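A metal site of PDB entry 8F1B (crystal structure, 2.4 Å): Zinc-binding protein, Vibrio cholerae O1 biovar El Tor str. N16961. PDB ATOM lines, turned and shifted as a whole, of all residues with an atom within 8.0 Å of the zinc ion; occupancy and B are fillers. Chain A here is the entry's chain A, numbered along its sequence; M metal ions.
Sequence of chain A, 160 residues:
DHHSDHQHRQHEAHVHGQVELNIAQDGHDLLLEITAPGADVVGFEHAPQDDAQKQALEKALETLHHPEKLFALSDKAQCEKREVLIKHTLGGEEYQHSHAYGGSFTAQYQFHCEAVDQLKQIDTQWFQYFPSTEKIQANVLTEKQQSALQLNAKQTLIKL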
ATOM      1  N   LYS A  59     -20.267   1.426  -0.372  1.00  0.00           N
ATOM      2  CA  LYS A  59     -21.317   2.345  -0.882  1.00  0.00           C
ATOM      3  C   LYS A  59     -21.075   3.742  -0.288  1.00  0.00           C
ATOM      4  O   LYS A  59     -21.035   4.719  -1.073  1.00  0.00           O
ATOM      5  CB  LYS A  59     -22.718   1.827  -0.561  1.00  0.00           C
ATOM      6  CG  LYS A  59     -23.785   2.306  -1.550  1.00  0.00           C
ATOM      7  CD  LYS A  59     -25.224   2.141  -1.100  1.00  0.00           C
ATOM      8  CE  LYS A  59     -25.863   3.436  -0.659  1.00  0.00           C
ATOM      9  NZ  LYS A  59     -27.184   3.218   0.000  1.00  0.00           N
ATOM     10  N   LEU A  61     -18.253   5.135   1.100  1.00  0.00           N
ATOM     11  CA  LEU A  61     -16.986   5.768   0.664  1.00  0.00           C
ATOM     12  C   LEU A  61     -17.149   6.263  -0.773  1.00  0.00           C
ATOM     13  O   LEU A  61     -16.646   7.335  -1.088  1.00  0.00           O
ATOM     14  CB  LEU A  61     -15.827   4.772   0.783  1.00  0.00           C
ATOM     15  CG  LEU A  61     -15.330   4.583   2.213  1.00  0.00           C
ATOM     16  CD1 LEU A  61     -14.534   3.289   2.360  1.00  0.00           C
ATOM     17  CD2 LEU A  61     -14.516   5.796   2.670  1.00  0.00           C
ATOM     18  N   GLU A  62     -17.846   5.501  -1.586  1.00  0.00           N
ATOM     19  CA  GLU A  62     -18.083   5.881  -2.995  1.00  0.00           C
ATOM     20  C   GLU A  62     -19.012   7.109  -3.015  1.00  0.00           C
ATOM     21  O   GLU A  62     -18.820   7.969  -3.879  1.00  0.00           O
ATOM     22  CB  GLU A  62     -18.619   4.679  -3.769  1.00  0.00           C
ATOM     23  CG  GLU A  62     -18.636   4.893  -5.272  1.00  0.00           C
ATOM     24  CD  GLU A  62     -19.839   5.701  -5.757  1.00  0.00           C
ATOM     25  OE1 GLU A  62     -20.860   5.680  -5.055  1.00  0.00           O
ATOM     26  OE2 GLU A  62     -19.739   6.345  -6.803  1.00  0.00           O
ATOM     27  N   THR A  63     -19.988   7.169  -2.129  1.00  0.00           N
ATOM     28  CA  THR A  63     -20.926   8.318  -2.047  1.00  0.00           C
ATOM     29  C   THR A  63     -20.162   9.589  -1.659  1.00  0.00           C
ATOM     30  O   THR A  63     -20.439  10.651  -2.261  1.00  0.00           O
ATOM     31  CB  THR A  63     -22.035   8.097  -1.026  1.00  0.00           C
ATOM     32  OG1 THR A  63     -22.847   7.041  -1.549  1.00  0.00           O
ATOM     33  CG2 THR A  63     -22.857   9.341  -0.799  1.00  0.00           C
ATOM     34  N   LEU A  64     -19.244   9.465  -0.708  1.00  0.00           N
ATOM     35  CA  LEU A  64     -18.578  10.637  -0.093  1.00  0.00           C
ATOM     36  C   LEU A  64     -17.693  11.363  -1.108  1.00  0.00           C
ATOM     37  O   LEU A  64     -17.284  12.471  -0.791  1.00  0.00           O
ATOM     38  CB  LEU A  64     -17.740  10.168   1.098  1.00  0.00           C
ATOM     39  CG  LEU A  64     -18.497   9.935   2.396  1.00  0.00           C
ATOM     40  CD1 LEU A  64     -17.525   9.601   3.525  1.00  0.00           C
ATOM     41  CD2 LEU A  64     -19.321  11.154   2.786  1.00  0.00           C
ATOM     42  N   HIS A  65     -17.382  10.780  -2.263  1.00  0.00           N
ATOM     43  CA  HIS A  65     -16.553  11.477  -3.285  1.00  0.00           C
ATOM     44  C   HIS A  65     -17.458  12.120  -4.348  1.00  0.00           C
ATOM     45  O   HIS A  65     -16.966  12.507  -5.384  1.00  0.00           O
ATOM     46  CB  HIS A  65     -15.444  10.579  -3.845  1.00  0.00           C
ATOM     47  CG  HIS A  65     -15.902   9.520  -4.789  1.00  0.00           C
ATOM     48  ND1 HIS A  65     -15.443   8.228  -4.701  1.00  0.00           N
ATOM     49  CD2 HIS A  65     -16.768   9.553  -5.835  1.00  0.00           C
ATOM     50  CE1 HIS A  65     -16.004   7.509  -5.643  1.00  0.00           C
ATOM     51  NE2 HIS A  65     -16.818   8.278  -6.348  1.00  0.00           N
ATOM     52  N   HIS A  66     -18.752  12.259  -4.062  1.00  0.00           N
ATOM     53  CA  HIS A  66     -19.693  12.992  -4.936  1.00  0.00           C
ATOM     54  C   HIS A  66     -20.326  14.105  -4.132  1.00  0.00           C
ATOM     55  O   HIS A  66     -21.507  14.059  -3.855  1.00  0.00           O
ATOM     56  CB  HIS A  66     -20.725  12.036  -5.529  1.00  0.00           C
ATOM     57  CG  HIS A  66     -20.145  11.030  -6.453  1.00  0.00           C
ATOM     58  ND1 HIS A  66     -19.538  11.376  -7.627  1.00  0.00           N
ATOM     59  CD2 HIS A  66     -20.098   9.681  -6.393  1.00  0.00           C
ATOM     60  CE1 HIS A  66     -19.119  10.284  -8.250  1.00  0.00           C
ATOM     61  NE2 HIS A  66     -19.451   9.230  -7.515  1.00  0.00           N
ATOM     62  N   GLU A  68     -21.066  16.819  -5.204  1.00  0.00           N
ATOM     63  CA  GLU A  68     -22.017  17.438  -6.163  1.00  0.00           C
ATOM     64  C   GLU A  68     -23.353  16.701  -6.087  1.00  0.00           C
ATOM     65  O   GLU A  68     -24.359  17.275  -6.550  1.00  0.00           O
ATOM     66  CB  GLU A  68     -21.409  17.488  -7.563  1.00  0.00           C
ATOM     67  CG  GLU A  68     -21.486  16.182  -8.305  1.00  0.00           C
ATOM     68  CD  GLU A  68     -20.451  15.135  -7.908  1.00  0.00           C
ATOM     69  OE1 GLU A  68     -19.650  15.402  -6.955  1.00  0.00           O
ATOM     70  OE2 GLU A  68     -20.443  14.065  -8.565  1.00  0.00           O
ATOM     71  N   LYS A  69     -23.402  15.489  -5.530  1.00  0.00           N
ATOM     72  CA  LYS A  69     -24.675  14.818  -5.193  1.00  0.00           C
ATOM     73  C   LYS A  69     -25.112  15.185  -3.778  1.00  0.00           C
ATOM     74  O   LYS A  69     -26.315  15.225  -3.528  1.00  0.00           O
ATOM     75  CB  LYS A  69     -24.568  13.296  -5.218  1.00  0.00           C
ATOM     76  CG  LYS A  69     -24.271  12.672  -6.562  1.00  0.00           C
ATOM     77  CD  LYS A  69     -24.570  11.179  -6.522  1.00  0.00           C
ATOM     78  CE  LYS A  69     -23.560  10.294  -7.216  1.00  0.00           C
ATOM     79  NZ  LYS A  69     -23.500  10.581  -8.667  1.00  0.00           N
ATOM     80  N   LYS A  81     -15.626  20.668  -9.296  1.00  0.00           N
ATOM     81  CA  LYS A  81     -14.980  20.046  -8.109  1.00  0.00           C
ATOM     82  C   LYS A  81     -13.471  20.236  -8.248  1.00  0.00           C
ATOM     83  O   LYS A  81     -12.926  19.903  -9.322  1.00  0.00           O
ATOM     84  CB  LYS A  81     -15.296  18.562  -7.945  1.00  0.00           C
ATOM     85  CG  LYS A  81     -16.746  18.199  -8.123  1.00  0.00           C
ATOM     86  CD  LYS A  81     -16.919  16.800  -8.663  1.00  0.00           C
ATOM     87  CE  LYS A  81     -16.237  15.768  -7.783  1.00  0.00           C
ATOM     88  NZ  LYS A  81     -16.571  14.388  -8.235  1.00  0.00           N
HETATM   89 ZN    ZN M   1     -18.290   7.576  -7.550  1.00  0.00          ZN
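ND1 of His 66 sits at hydrogen-bond distance from OE2 of Glu 68. The backbone carbonyl oxygen of His 65 is in hydrogen-bond range of the side-chain amino group of Lys 81, at 3.4 Å.
The zinc ion is bound by a ring nitrogen (NE2) of His 66 (2.0 Å). NE2 of His 65 is bound to the zinc ion (2.0 Å). OE2 of Glu 62 binds the zinc ion, at 2.0 Å. The zinc ion has three donor atoms within binding distance.
Of the 10 residues printed, 3 come within 4 Å of the zinc ion. Along chain A the residues within 4 Å of the zinc ion span positions 62 to 66. The nearest printed residue that does not touch the zinc ion is Thr 63 (5.7 Å).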
